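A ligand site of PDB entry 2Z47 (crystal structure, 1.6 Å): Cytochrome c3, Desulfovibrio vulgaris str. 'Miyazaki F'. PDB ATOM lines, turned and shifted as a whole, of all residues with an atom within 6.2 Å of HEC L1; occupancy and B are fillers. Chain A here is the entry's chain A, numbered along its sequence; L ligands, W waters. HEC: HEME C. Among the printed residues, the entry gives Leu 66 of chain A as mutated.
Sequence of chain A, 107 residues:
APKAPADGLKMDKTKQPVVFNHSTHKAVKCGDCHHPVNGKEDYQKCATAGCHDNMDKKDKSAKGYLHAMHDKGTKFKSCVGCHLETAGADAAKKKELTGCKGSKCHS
O1D of HEC L1 is in hydrogen-bond range of N of Lys 13 (2.8 Å). An iron atom (FE) of HEC L1 is bound by a ring nitrogen (NE2) of His 70. The backbone NH of Thr 14 sits at hydrogen-bond distance from an oxygen (O2D) of HEC L1 (2.8 Å). A ring nitrogen (NE2) of His 106 is bound to an iron atom (FE) of HEC L1 (2.0 Å). The side-chain sulfur (SG) of Cys 100 is covalently linked to a carbon (CAB) of HEC L1 (1.8 Å). A ring nitrogen (NE2) of His 83 binds an iron atom (FE) of HEC L2, at 2.0 Å. A carbon (CAC) of HEC L1 is bonded to the side-chain sulfur of Cys 105, 1.8 Å away. CAB of HEC L2 is covalently linked to SG of Cys 79 (1.8 Å). O2D of HEC L1 sits close to O of Met 11, at 3.1 Å. N of Lys 15 lies within hydrogen-bond range of O1A of HEC L1 (2.9 Å). O1D of HEC L1 lies within hydrogen-bond range of OH of Tyr 65 (2.6 Å). O2D of HEC L1 is in hydrogen-bond range of OG1 of Thr 14 (2.7 Å).
The backbone carbonyl oxygen (O) of Val 18 sits at hydrogen-bond distance from the backbone NH (N) of Met 11, at 2.9 Å. The backbone NH (N) of Gln 16 sits at hydrogen-bond distance from the side-chain hydroxyl (OG1) of Thr 14. The side-chain hydroxyl (OG) of Ser 103 is in hydrogen-bond range of the backbone NH (N) of His 106 (3.1 Å). O of Gly 99 lies within hydrogen-bond range of OG of Ser 103 (2.7 Å). O of Met 69 sits at hydrogen-bond distance from N of Val 80. The backbone carbonyl oxygen (O) of Leu 66 is in hydrogen-bond range of a ring nitrogen (ND1) of His 70 (2.8 Å). The backbone NH (N) of Cys 79 lies close to the backbone carbonyl oxygen (O) of Met 69, 3.2 Å away. The backbone NH (N) of Cys 105 sits close to the side-chain hydroxyl (OG) of Ser 103 (3.2 Å).
Merely in contact with HEC L1: Asp 12 (3.4 Å), Gln 16 (3.6 Å), Pro 17 (3.4 Å), Val 18 (3.5 Å), Lys 57 (3.4 Å), Leu 66 (3.6 Å), Met 69 (3.9 Å), Cys 79 (3.8 Å), Val 80 (3.8 Å), His 83 (3.3 Å), Leu 97 (3.3 Å), Thr 98 (3.5 Å) and Gly 99 (3.6 Å). Within 4 Å of HEC L1: Met 11, Asp 12, Lys 13, Thr 14, Lys 15, Gln 16, Pro 17, Val 18, Lys 57, Tyr 65, Leu 66, Met 69, His 70, Cys 79, Val 80, His 83, Leu 97, Thr 98, Gly 99, Cys 100, Cys 105 and His 106. The nearest printed residue that does not touch HEC L1 is Ser 103 (4.1 Å).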
ATOM      1  N   MET A  11     -13.328 -17.367  11.918  1.00  0.00           N
ATOM      2  CA  MET A  11     -13.397 -16.884  10.540  1.00  0.00           C
ATOM      3  C   MET A  11     -14.716 -17.494  10.086  1.00  0.00           C
ATOM      4  O   MET A  11     -14.786 -18.688   9.811  1.00  0.00           O
ATOM      5  CB  MET A  11     -12.213 -17.435   9.729  1.00  0.00           C
ATOM      6  CG  MET A  11     -10.856 -16.943  10.241  1.00  0.00           C
ATOM      7  SD  MET A  11      -9.433 -17.526   9.300  1.00  0.00           S
ATOM      8  CE  MET A  11      -9.494 -16.437   7.859  1.00  0.00           C
ATOM      9  N   ASP A  12     -15.760 -16.676  10.043  1.00  0.00           N
ATOM     10  CA  ASP A  12     -17.077 -17.177   9.683  1.00  0.00           C
ATOM     11  C   ASP A  12     -17.804 -16.454   8.560  1.00  0.00           C
ATOM     12  O   ASP A  12     -18.964 -16.066   8.718  1.00  0.00           O
ATOM     13  CB  ASP A  12     -17.983 -17.174  10.929  1.00  0.00           C
ATOM     14  CG  ASP A  12     -17.983 -15.830  11.636  1.00  0.00           C
ATOM     15  OD1 ASP A  12     -17.564 -14.824  11.023  1.00  0.00           O
ATOM     16  OD2 ASP A  12     -18.411 -15.776  12.811  1.00  0.00           O
ATOM     17  N   LYS A  13     -17.140 -16.283   7.424  1.00  0.00           N
ATOM     18  CA  LYS A  13     -17.776 -15.624   6.290  1.00  0.00           C
ATOM     19  C   LYS A  13     -18.549 -16.658   5.478  1.00  0.00           C
ATOM     20  O   LYS A  13     -19.351 -16.314   4.611  1.00  0.00           O
ATOM     21  CB  LYS A  13     -16.725 -14.964   5.401  1.00  0.00           C
ATOM     22  CG  LYS A  13     -15.786 -14.016   6.132  1.00  0.00           C
ATOM     23  CD  LYS A  13     -16.481 -12.747   6.597  1.00  0.00           C
ATOM     24  CE  LYS A  13     -16.866 -11.863   5.418  1.00  0.00           C
ATOM     25  NZ  LYS A  13     -17.362 -10.537   5.873  1.00  0.00           N
ATOM     26  N   THR A  14     -18.319 -17.940   5.783  1.00  0.00           N
ATOM     27  CA  THR A  14     -18.963 -19.029   5.055  1.00  0.00           C
ATOM     28  C   THR A  14     -19.724 -20.009   5.946  1.00  0.00           C
ATOM     29  O   THR A  14     -19.867 -19.807   7.146  1.00  0.00           O
ATOM     30  CB  THR A  14     -17.926 -19.844   4.255  1.00  0.00           C
ATOM     31  OG1 THR A  14     -17.251 -20.752   5.137  1.00  0.00           O
ATOM     32  CG2 THR A  14     -16.900 -18.907   3.624  1.00  0.00           C
ATOM     33  N   LYS A  15     -20.226 -21.080   5.334  1.00  0.00           N
ATOM     34  CA  LYS A  15     -20.973 -22.101   6.067  1.00  0.00           C
ATOM     35  C   LYS A  15     -20.060 -23.144   6.705  1.00  0.00           C
ATOM     36  O   LYS A  15     -20.528 -24.078   7.351  1.00  0.00           O
ATOM     37  CB  LYS A  15     -21.990 -22.794   5.153  1.00  0.00           C
ATOM     38  CG  LYS A  15     -23.129 -21.875   4.704  1.00  0.00           C
ATOM     39  CD  LYS A  15     -24.281 -22.688   4.134  1.00  0.00           C
ATOM     40  CE  LYS A  15     -25.439 -21.784   3.744  1.00  0.00           C
ATOM     41  NZ  LYS A  15     -26.601 -22.563   3.246  1.00  0.00           N
ATOM     42  N   GLN A  16     -18.754 -22.969   6.521  1.00  0.00           N
ATOM     43  CA  GLN A  16     -17.776 -23.879   7.102  1.00  0.00           C
ATOM     44  C   GLN A  16     -16.748 -23.023   7.845  1.00  0.00           C
ATOM     45  O   GLN A  16     -15.583 -22.969   7.463  1.00  0.00           O
ATOM     46  CB  GLN A  16     -17.083 -24.706   6.016  1.00  0.00           C
ATOM     47  CG  GLN A  16     -17.987 -25.710   5.320  1.00  0.00           C
ATOM     48  CD  GLN A  16     -18.621 -26.692   6.291  1.00  0.00           C
ATOM     49  OE1 GLN A  16     -17.984 -27.167   7.228  1.00  0.00           O
ATOM     50  NE2 GLN A  16     -19.893 -27.004   6.058  1.00  0.00           N
ATOM     51  N   PRO A  17     -17.188 -22.337   8.913  1.00  0.00           N
ATOM     52  CA  PRO A  17     -16.291 -21.490   9.688  1.00  0.00           C
ATOM     53  C   PRO A  17     -15.072 -22.231  10.208  1.00  0.00           C
ATOM     54  O   PRO A  17     -15.127 -23.438  10.481  1.00  0.00           O
ATOM     55  CB  PRO A  17     -17.186 -20.983  10.822  1.00  0.00           C
ATOM     56  CG  PRO A  17     -18.156 -22.101  10.991  1.00  0.00           C
ATOM     57  CD  PRO A  17     -18.502 -22.436   9.568  1.00  0.00           C
ATOM     58  N   VAL A  18     -13.962 -21.505  10.337  1.00  0.00           N
ATOM     59  CA  VAL A  18     -12.712 -22.070  10.813  1.00  0.00           C
ATOM     60  C   VAL A  18     -12.142 -21.194  11.919  1.00  0.00           C
ATOM     61  O   VAL A  18     -12.164 -19.973  11.819  1.00  0.00           O
ATOM     62  CB  VAL A  18     -11.681 -22.159   9.653  1.00  0.00           C
ATOM     63  CG1 VAL A  18     -10.336 -22.646  10.170  1.00  0.00           C
ATOM     64  CG2 VAL A  18     -12.216 -23.090   8.572  1.00  0.00           C
ATOM     65  N   LYS A  57     -16.614 -19.239  -4.967  1.00  0.00           N
ATOM     66  CA  LYS A  57     -15.634 -20.322  -4.885  1.00  0.00           C
ATOM     67  C   LYS A  57     -14.674 -20.405  -6.063  1.00  0.00           C
ATOM     68  O   LYS A  57     -13.561 -20.913  -5.930  1.00  0.00           O
ATOM     69  CB  LYS A  57     -16.355 -21.666  -4.758  1.00  0.00           C
ATOM     70  CG  LYS A  57     -17.268 -21.779  -3.545  1.00  0.00           C
ATOM     71  CD  LYS A  57     -17.835 -23.182  -3.409  1.00  0.00           C
ATOM     72  CE  LYS A  57     -16.745 -24.214  -3.159  1.00  0.00           C
ATOM     73  NZ  LYS A  57     -17.297 -25.549  -2.794  1.00  0.00           N
ATOM     74  N   TYR A  65     -11.751 -14.753  -1.705  1.00  0.00           N
ATOM     75  CA  TYR A  65     -11.559 -15.097  -0.290  1.00  0.00           C
ATOM     76  C   TYR A  65     -11.075 -16.533  -0.099  1.00  0.00           C
ATOM     77  O   TYR A  65     -10.062 -16.775   0.552  1.00  0.00           O
ATOM     78  CB  TYR A  65     -12.875 -14.889   0.466  1.00  0.00           C
ATOM     79  CG  TYR A  65     -12.829 -15.214   1.933  1.00  0.00           C
ATOM     80  CD1 TYR A  65     -13.556 -16.282   2.454  1.00  0.00           C
ATOM     81  CD2 TYR A  65     -12.076 -14.440   2.816  1.00  0.00           C
ATOM     82  CE1 TYR A  65     -13.543 -16.573   3.817  1.00  0.00           C
ATOM     83  CE2 TYR A  65     -12.051 -14.722   4.182  1.00  0.00           C
ATOM     84  CZ  TYR A  65     -12.790 -15.793   4.681  1.00  0.00           C
ATOM     85  OH  TYR A  65     -12.776 -16.068   6.028  1.00  0.00           O
ATOM     86  N   LEU A  66     -11.802 -17.496  -0.673  1.00  0.00           N
ATOM     87  CA  LEU A  66     -11.426 -18.893  -0.520  1.00  0.00           C
ATOM     88  C   LEU A  66     -10.078 -19.211  -1.173  1.00  0.00           C
ATOM     89  O   LEU A  66      -9.316 -20.034  -0.665  1.00  0.00           O
ATOM     90  CB  LEU A  66     -12.538 -19.785  -1.094  1.00  0.00           C
ATOM     91  CG  LEU A  66     -13.872 -19.620  -0.361  1.00  0.00           C
ATOM     92  CD1 LEU A  66     -14.942 -20.442  -1.051  1.00  0.00           C
ATOM     93  CD2 LEU A  66     -13.711 -20.063   1.089  1.00  0.00           C
ATOM     94  N   MET A  69      -7.161 -18.630   1.103  1.00  0.00           N
ATOM     95  CA  MET A  69      -7.010 -19.566   2.222  1.00  0.00           C
ATOM     96  C   MET A  69      -6.614 -20.974   1.818  1.00  0.00           C
ATOM     97  O   MET A  69      -6.030 -21.698   2.621  1.00  0.00           O
ATOM     98  CB  MET A  69      -8.315 -19.663   3.012  1.00  0.00           C
ATOM     99  CG  MET A  69      -8.926 -18.332   3.399  1.00  0.00           C
ATOM    100  SD  MET A  69      -7.840 -17.326   4.393  1.00  0.00           S
ATOM    101  CE  MET A  69      -8.645 -15.734   4.236  1.00  0.00           C
ATOM    102  N   HIS A  70      -6.934 -21.368   0.586  1.00  0.00           N
ATOM    103  CA  HIS A  70      -6.675 -22.734   0.146  1.00  0.00           C
ATOM    104  C   HIS A  70      -5.662 -23.061  -0.948  1.00  0.00           C
ATOM    105  O   HIS A  70      -5.091 -24.146  -0.928  1.00  0.00           O
ATOM    106  CB  HIS A  70      -7.981 -23.403  -0.294  1.00  0.00           C
ATOM    107  CG  HIS A  70      -9.081 -23.375   0.715  1.00  0.00           C
ATOM    108  ND1 HIS A  70      -9.913 -22.295   0.889  1.00  0.00           N
ATOM    109  CD2 HIS A  70      -9.493 -24.313   1.599  1.00  0.00           C
ATOM    110  CE1 HIS A  70     -10.796 -22.564   1.826  1.00  0.00           C
ATOM    111  NE2 HIS A  70     -10.567 -23.785   2.285  1.00  0.00           N
ATOM    112  N   CYS A  79      -3.246 -20.689   3.890  1.00  0.00           N
ATOM    113  CA  CYS A  79      -3.351 -21.593   5.036  1.00  0.00           C
ATOM    114  C   CYS A  79      -2.914 -22.995   4.623  1.00  0.00           C
ATOM    115  O   CYS A  79      -1.993 -23.576   5.187  1.00  0.00           O
ATOM    116  CB  CYS A  79      -4.784 -21.673   5.543  1.00  0.00           C
ATOM    117  SG  CYS A  79      -5.639 -20.092   5.854  1.00  0.00           S
ATOM    118  N   VAL A  80      -3.611 -23.523   3.623  1.00  0.00           N
ATOM    119  CA  VAL A  80      -3.323 -24.867   3.126  1.00  0.00           C
ATOM    120  C   VAL A  80      -1.931 -24.961   2.517  1.00  0.00           C
ATOM    121  O   VAL A  80      -1.219 -25.941   2.752  1.00  0.00           O
ATOM    122  CB  VAL A  80      -4.374 -25.296   2.082  1.00  0.00           C
ATOM    123  CG1 VAL A  80      -4.013 -26.659   1.505  1.00  0.00           C
ATOM    124  CG2 VAL A  80      -5.750 -25.329   2.726  1.00  0.00           C
ATOM    125  N   HIS A  83       0.593 -25.189   5.255  1.00  0.00           N
ATOM    126  CA  HIS A  83       0.409 -26.452   5.974  1.00  0.00           C
ATOM    127  C   HIS A  83       0.930 -27.639   5.174  1.00  0.00           C
ATOM    128  O   HIS A  83       1.443 -28.610   5.740  1.00  0.00           O
ATOM    129  CB  HIS A  83      -1.062 -26.662   6.330  1.00  0.00           C
ATOM    130  CG  HIS A  83      -1.553 -25.778   7.437  1.00  0.00           C
ATOM    131  ND1 HIS A  83      -2.780 -25.949   8.037  1.00  0.00           N
ATOM    132  CD2 HIS A  83      -0.972 -24.724   8.064  1.00  0.00           C
ATOM    133  CE1 HIS A  83      -2.945 -25.037   8.977  1.00  0.00           C
ATOM    134  NE2 HIS A  83      -1.858 -24.280   9.011  1.00  0.00           N
ATOM    135  N   LYS A  95      -3.450 -34.952   6.918  1.00  0.00           N
ATOM    136  CA  LYS A  95      -4.883 -35.058   7.188  1.00  0.00           C
ATOM    137  C   LYS A  95      -5.293 -33.958   8.158  1.00  0.00           C
ATOM    138  O   LYS A  95      -6.249 -33.215   7.924  1.00  0.00           O
ATOM    139  CB  LYS A  95      -5.200 -36.424   7.787  1.00  0.00           C
ATOM    140  CG  LYS A  95      -6.668 -36.617   8.158  1.00  0.00           C
ATOM    141  CD  LYS A  95      -7.564 -36.566   6.937  1.00  0.00           C
ATOM    142  CE  LYS A  95      -8.990 -36.958   7.280  1.00  0.00           C
ATOM    143  NZ  LYS A  95      -9.869 -36.937   6.081  1.00  0.00           N
ATOM    144  N   GLU A  96      -4.557 -33.865   9.259  1.00  0.00           N
ATOM    145  CA  GLU A  96      -4.808 -32.895  10.301  1.00  0.00           C
ATOM    146  C   GLU A  96      -4.730 -31.428   9.843  1.00  0.00           C
ATOM    147  O   GLU A  96      -5.575 -30.615  10.220  1.00  0.00           O
ATOM    148  CB  GLU A  96      -3.811 -33.132  11.455  1.00  0.00           C
ATOM    149  CG  GLU A  96      -3.525 -31.925  12.332  1.00  0.00           C
ATOM    150  CD  GLU A  96      -2.440 -32.204  13.366  1.00  0.00           C
ATOM    151  OE1 GLU A  96      -1.950 -31.227  13.983  1.00  0.00           O
ATOM    152  OE2 GLU A  96      -2.082 -33.377  13.554  1.00  0.00           O
ATOM    153  N   LEU A  97      -3.731 -31.106   9.023  1.00  0.00           N
ATOM    154  CA  LEU A  97      -3.542 -29.723   8.579  1.00  0.00           C
ATOM    155  C   LEU A  97      -4.010 -29.341   7.182  1.00  0.00           C
ATOM    156  O   LEU A  97      -4.120 -28.145   6.890  1.00  0.00           O
ATOM    157  CB  LEU A  97      -2.065 -29.352   8.718  1.00  0.00           C
ATOM    158  CG  LEU A  97      -1.411 -29.614  10.072  1.00  0.00           C
ATOM    159  CD1 LEU A  97       0.096 -29.405   9.955  1.00  0.00           C
ATOM    160  CD2 LEU A  97      -2.013 -28.699  11.129  1.00  0.00           C
ATOM    161  N   THR A  98      -4.283 -30.313   6.321  1.00  0.00           N
ATOM    162  CA  THR A  98      -4.704 -29.968   4.954  1.00  0.00           C
ATOM    163  C   THR A  98      -5.957 -30.671   4.460  1.00  0.00           C
ATOM    164  O   THR A  98      -6.437 -30.374   3.362  1.00  0.00           O
ATOM    165  CB  THR A  98      -3.566 -30.231   3.937  1.00  0.00           C
ATOM    166  OG1 THR A  98      -3.386 -31.639   3.759  1.00  0.00           O
ATOM    167  CG2 THR A  98      -2.256 -29.631   4.430  1.00  0.00           C
ATOM    168  N   GLY A  99      -6.494 -31.593   5.248  1.00  0.00           N
ATOM    169  CA  GLY A  99      -7.684 -32.318   4.829  1.00  0.00           C
ATOM    170  C   GLY A  99      -8.922 -31.444   4.662  1.00  0.00           C
ATOM    171  O   GLY A  99      -9.148 -30.533   5.457  1.00  0.00           O
ATOM    172  N   CYS A 100      -9.720 -31.740   3.639  1.00  0.00           N
ATOM    173  CA  CYS A 100     -10.941 -30.988   3.373  1.00  0.00           C
ATOM    174  C   CYS A 100     -12.032 -31.396   4.358  1.00  0.00           C
ATOM    175  O   CYS A 100     -13.024 -30.686   4.553  1.00  0.00           O
ATOM    176  CB  CYS A 100     -11.417 -31.235   1.938  1.00  0.00           C
ATOM    177  SG  CYS A 100     -10.133 -30.909   0.694  1.00  0.00           S
ATOM    178  N   LYS A 101     -11.846 -32.557   4.961  1.00  0.00           N
ATOM    179  CA  LYS A 101     -12.769 -33.077   5.951  1.00  0.00           C
ATOM    180  C   LYS A 101     -11.960 -33.873   6.956  1.00  0.00           C
ATOM    181  O   LYS A 101     -10.931 -34.460   6.608  1.00  0.00           O
ATOM    182  CB  LYS A 101     -13.819 -33.984   5.287  1.00  0.00           C
ATOM    183  CG  LYS A 101     -13.276 -35.247   4.662  1.00  0.00           C
ATOM    184  CD  LYS A 101     -14.393 -36.091   4.071  1.00  0.00           C
ATOM    185  CE  LYS A 101     -13.872 -37.401   3.515  1.00  0.00           C
ATOM    186  NZ  LYS A 101     -13.203 -38.221   4.570  1.00  0.00           N
ATOM    187  N   SER A 103     -10.224 -32.651   9.329  1.00  0.00           N
ATOM    188  CA  SER A 103      -8.999 -31.911   9.636  1.00  0.00           C
ATOM    189  C   SER A 103      -9.264 -30.947  10.781  1.00  0.00           C
ATOM    190  O   SER A 103     -10.398 -30.820  11.247  1.00  0.00           O
ATOM    191  CB  SER A 103      -8.500 -31.130   8.412  1.00  0.00           C
ATOM    192  OG  SER A 103      -9.364 -30.044   8.109  1.00  0.00           O
ATOM    193  N   LYS A 104      -8.219 -30.260  11.224  1.00  0.00           N
ATOM    194  CA  LYS A 104      -8.377 -29.297  12.313  1.00  0.00           C
ATOM    195  C   LYS A 104      -9.054 -28.023  11.841  1.00  0.00           C
ATOM    196  O   LYS A 104      -9.418 -27.167  12.644  1.00  0.00           O
ATOM    197  CB  LYS A 104      -7.016 -28.985  12.939  1.00  0.00           C
ATOM    198  CG  LYS A 104      -6.464 -30.155  13.737  1.00  0.00           C
ATOM    199  CD  LYS A 104      -5.215 -29.777  14.522  1.00  0.00           C
ATOM    200  CE  LYS A 104      -4.783 -30.916  15.426  1.00  0.00           C
ATOM    201  NZ  LYS A 104      -3.568 -30.568  16.223  1.00  0.00           N
ATOM    202  N   CYS A 105      -9.218 -27.892  10.528  1.00  0.00           N
ATOM    203  CA  CYS A 105      -9.895 -26.718   9.964  1.00  0.00           C
ATOM    204  C   CYS A 105     -11.363 -27.053   9.731  1.00  0.00           C
ATOM    205  O   CYS A 105     -12.254 -26.305  10.142  1.00  0.00           O
ATOM    206  CB  CYS A 105      -9.239 -26.294   8.652  1.00  0.00           C
ATOM    207  SG  CYS A 105      -7.566 -25.619   8.834  1.00  0.00           S
ATOM    208  N   HIS A 106     -11.603 -28.180   9.063  1.00  0.00           N
ATOM    209  CA  HIS A 106     -12.969 -28.629   8.772  1.00  0.00           C
ATOM    210  C   HIS A 106     -13.142 -30.031   9.346  1.00  0.00           C
ATOM    211  O   HIS A 106     -12.592 -30.993   8.808  1.00  0.00           O
ATOM    212  CB  HIS A 106     -13.220 -28.668   7.256  1.00  0.00           C
ATOM    213  CG  HIS A 106     -12.979 -27.364   6.548  1.00  0.00           C
ATOM    214  ND1 HIS A 106     -13.615 -26.198   6.897  1.00  0.00           N
ATOM    215  CD2 HIS A 106     -12.204 -27.071   5.475  1.00  0.00           C
ATOM    216  CE1 HIS A 106     -13.258 -25.234   6.065  1.00  0.00           C
ATOM    217  NE2 HIS A 106     -12.395 -25.736   5.184  1.00  0.00           N
HETATM  218 FE   HEC L   1     -11.516 -24.766   3.682  1.00  0.00          FE
HETATM  219  CHA HEC L   1     -13.782 -22.282   3.891  1.00  0.00           C
HETATM  220  CHB HEC L   1     -13.214 -26.126   1.111  1.00  0.00           C
HETATM  221  CHC HEC L   1      -9.297 -27.360   3.588  1.00  0.00           C
HETATM  222  CHD HEC L   1      -9.524 -23.151   5.902  1.00  0.00           C
HETATM  223  NA  HEC L   1     -13.346 -24.352   2.729  1.00  0.00           N
HETATM  224  C1A HEC L   1     -14.114 -23.296   2.988  1.00  0.00           C
HETATM  225  C2A HEC L   1     -15.270 -23.379   2.225  1.00  0.00           C
HETATM  226  C3A HEC L   1     -15.062 -24.457   1.361  1.00  0.00           C
HETATM  227  C4A HEC L   1     -13.841 -25.023   1.713  1.00  0.00           C
HETATM  228  CMA HEC L   1     -15.971 -24.912   0.222  1.00  0.00           C
HETATM  229  CAA HEC L   1     -16.502 -22.497   2.279  1.00  0.00           C
HETATM  230  CBA HEC L   1     -17.786 -23.308   2.432  1.00  0.00           C
HETATM  231  CGA HEC L   1     -18.994 -22.604   1.850  1.00  0.00           C
HETATM  232  O1A HEC L   1     -19.706 -21.898   2.598  1.00  0.00           O
HETATM  233  O2A HEC L   1     -19.240 -22.764   0.642  1.00  0.00           O
HETATM  234  NB  HEC L   1     -11.268 -26.508   2.507  1.00  0.00           N
HETATM  235  C1B HEC L   1     -12.018 -26.801   1.452  1.00  0.00           C
HETATM  236  C2B HEC L   1     -11.450 -27.841   0.735  1.00  0.00           C
HETATM  237  C3B HEC L   1     -10.352 -28.252   1.490  1.00  0.00           C
HETATM  238  C4B HEC L   1     -10.271 -27.388   2.575  1.00  0.00           C
HETATM  239  CMB HEC L   1     -11.950 -28.390  -0.590  1.00  0.00           C
HETATM  240  CAB HEC L   1      -9.461 -29.287   1.203  1.00  0.00           C
HETATM  241  CBB HEC L   1      -8.585 -29.174   0.043  1.00  0.00           C
HETATM  242  NC  HEC L   1      -9.700 -25.216   4.655  1.00  0.00           N
HETATM  243  C1C HEC L   1      -9.036 -26.372   4.547  1.00  0.00           C
HETATM  244  C2C HEC L   1      -8.056 -26.426   5.515  1.00  0.00           C
HETATM  245  C3C HEC L   1      -8.107 -25.212   6.185  1.00  0.00           C
HETATM  246  C4C HEC L   1      -9.119 -24.470   5.587  1.00  0.00           C
HETATM  247  CMC HEC L   1      -7.126 -27.593   5.771  1.00  0.00           C
HETATM  248  CAC HEC L   1      -7.298 -24.779   7.237  1.00  0.00           C
HETATM  249  CBC HEC L   1      -5.853 -24.920   7.197  1.00  0.00           C
HETATM  250  ND  HEC L   1     -11.612 -22.952   4.706  1.00  0.00           N
HETATM  251  C1D HEC L   1     -10.659 -22.445   5.495  1.00  0.00           C
HETATM  252  C2D HEC L   1     -11.003 -21.150   5.864  1.00  0.00           C
HETATM  253  C3D HEC L   1     -12.288 -20.972   5.358  1.00  0.00           C
HETATM  254  C4D HEC L   1     -12.603 -22.092   4.632  1.00  0.00           C
HETATM  255  CMD HEC L   1     -10.138 -20.160   6.630  1.00  0.00           C
HETATM  256  CAD HEC L   1     -13.241 -19.809   5.528  1.00  0.00           C
HETATM  257  CBD HEC L   1     -13.951 -19.834   6.876  1.00  0.00           C
HETATM  258  CGD HEC L   1     -15.050 -18.806   6.937  1.00  0.00           C
HETATM  259  O1D HEC L   1     -14.734 -17.606   6.801  1.00  0.00           O
HETATM  260  O2D HEC L   1     -16.223 -19.191   7.119  1.00  0.00           O
HETATM  261 FE   HEC L   2      -1.725 -22.817  10.396  1.00  0.00          FE
HETATM  262  CHA HEC L   2      -1.278 -25.134  12.821  1.00  0.00           C
HETATM  263  CHB HEC L   2      -5.076 -23.064  10.846  1.00  0.00           C
HETATM  264  CHC HEC L   2      -2.185 -20.429   8.065  1.00  0.00           C
HETATM  265  CHD HEC L   2       1.607 -22.737   9.845  1.00  0.00           C
HETATM  266  NA  HEC L   2      -2.997 -23.899  11.699  1.00  0.00           N
HETATM  267  C1A HEC L   2      -2.608 -24.820  12.565  1.00  0.00           C
HETATM  268  C2A HEC L   2      -3.695 -25.438  13.144  1.00  0.00           C
HETATM  269  C3A HEC L   2      -4.815 -24.885  12.525  1.00  0.00           C
HETATM  270  C4A HEC L   2      -4.328 -23.921  11.658  1.00  0.00           C
HETATM  271  CMA HEC L   2      -6.267 -25.261  12.759  1.00  0.00           C
HETATM  272  CAA HEC L   2      -3.649 -26.470  14.248  1.00  0.00           C
HETATM  273  CBA HEC L   2      -3.459 -25.842  15.615  1.00  0.00           C
HETATM  274  CGA HEC L   2      -4.651 -24.991  16.013  1.00  0.00           C
HETATM  275  O1A HEC L   2      -5.758 -25.548  16.173  1.00  0.00           O
HETATM  276  O2A HEC L   2      -4.484 -23.762  16.150  1.00  0.00           O
HETATM  277  NB  HEC L   2      -3.393 -21.826   9.618  1.00  0.00           N
HETATM  278  C1B HEC L   2      -4.663 -22.093   9.920  1.00  0.00           C
HETATM  279  C2B HEC L   2      -5.514 -21.281   9.172  1.00  0.00           C
HETATM  280  C3B HEC L   2      -4.665 -20.519   8.370  1.00  0.00           C
HETATM  281  C4B HEC L   2      -3.373 -20.912   8.666  1.00  0.00           C
HETATM  282  CMB HEC L   2      -7.037 -21.282   9.235  1.00  0.00           C
HETATM  283  CAB HEC L   2      -4.993 -19.502   7.468  1.00  0.00           C
HETATM  284  CBB HEC L   2      -6.145 -18.633   7.672  1.00  0.00           C
HETATM  285  NC  HEC L   2      -0.456 -21.715   9.140  1.00  0.00           N
HETATM  286  C1C HEC L   2      -0.850 -20.820   8.256  1.00  0.00           C
HETATM  287  C2C HEC L   2       0.239 -20.339   7.532  1.00  0.00           C
HETATM  288  C3C HEC L   2       1.337 -21.062   8.019  1.00  0.00           C
HETATM  289  C4C HEC L   2       0.851 -21.869   9.036  1.00  0.00           C
HETATM  290  CMC HEC L   2       0.136 -19.284   6.448  1.00  0.00           C
HETATM  291  CAC HEC L   2       2.675 -20.993   7.636  1.00  0.00           C
HETATM  292  CBC HEC L   2       3.243 -19.910   6.822  1.00  0.00           C
HETATM  293  ND  HEC L   2      -0.058 -23.723  11.281  1.00  0.00           N
HETATM  294  C1D HEC L   2       1.199 -23.585  10.890  1.00  0.00           C
HETATM  295  C2D HEC L   2       2.023 -24.377  11.656  1.00  0.00           C
HETATM  296  C3D HEC L   2       1.174 -25.086  12.493  1.00  0.00           C
HETATM  297  C4D HEC L   2      -0.100 -24.650  12.220  1.00  0.00           C
HETATM  298  CMD HEC L   2       3.537 -24.433  11.575  1.00  0.00           C
HETATM  299  CAD HEC L   2       1.429 -26.178  13.511  1.00  0.00           C
HETATM  300  CBD HEC L   2       1.727 -27.523  12.868  1.00  0.00           C
HETATM  301  CGD HEC L   2       1.327 -28.676  13.761  1.00  0.00           C
HETATM  302  O1D HEC L   2       1.652 -29.832  13.434  1.00  0.00           O
HETATM  303  O2D HEC L   2       0.663 -28.428  14.791  1.00  0.00           O
HETATM  304  O   HOH W   1     -15.133 -27.065  -2.143  1.00  0.00           O
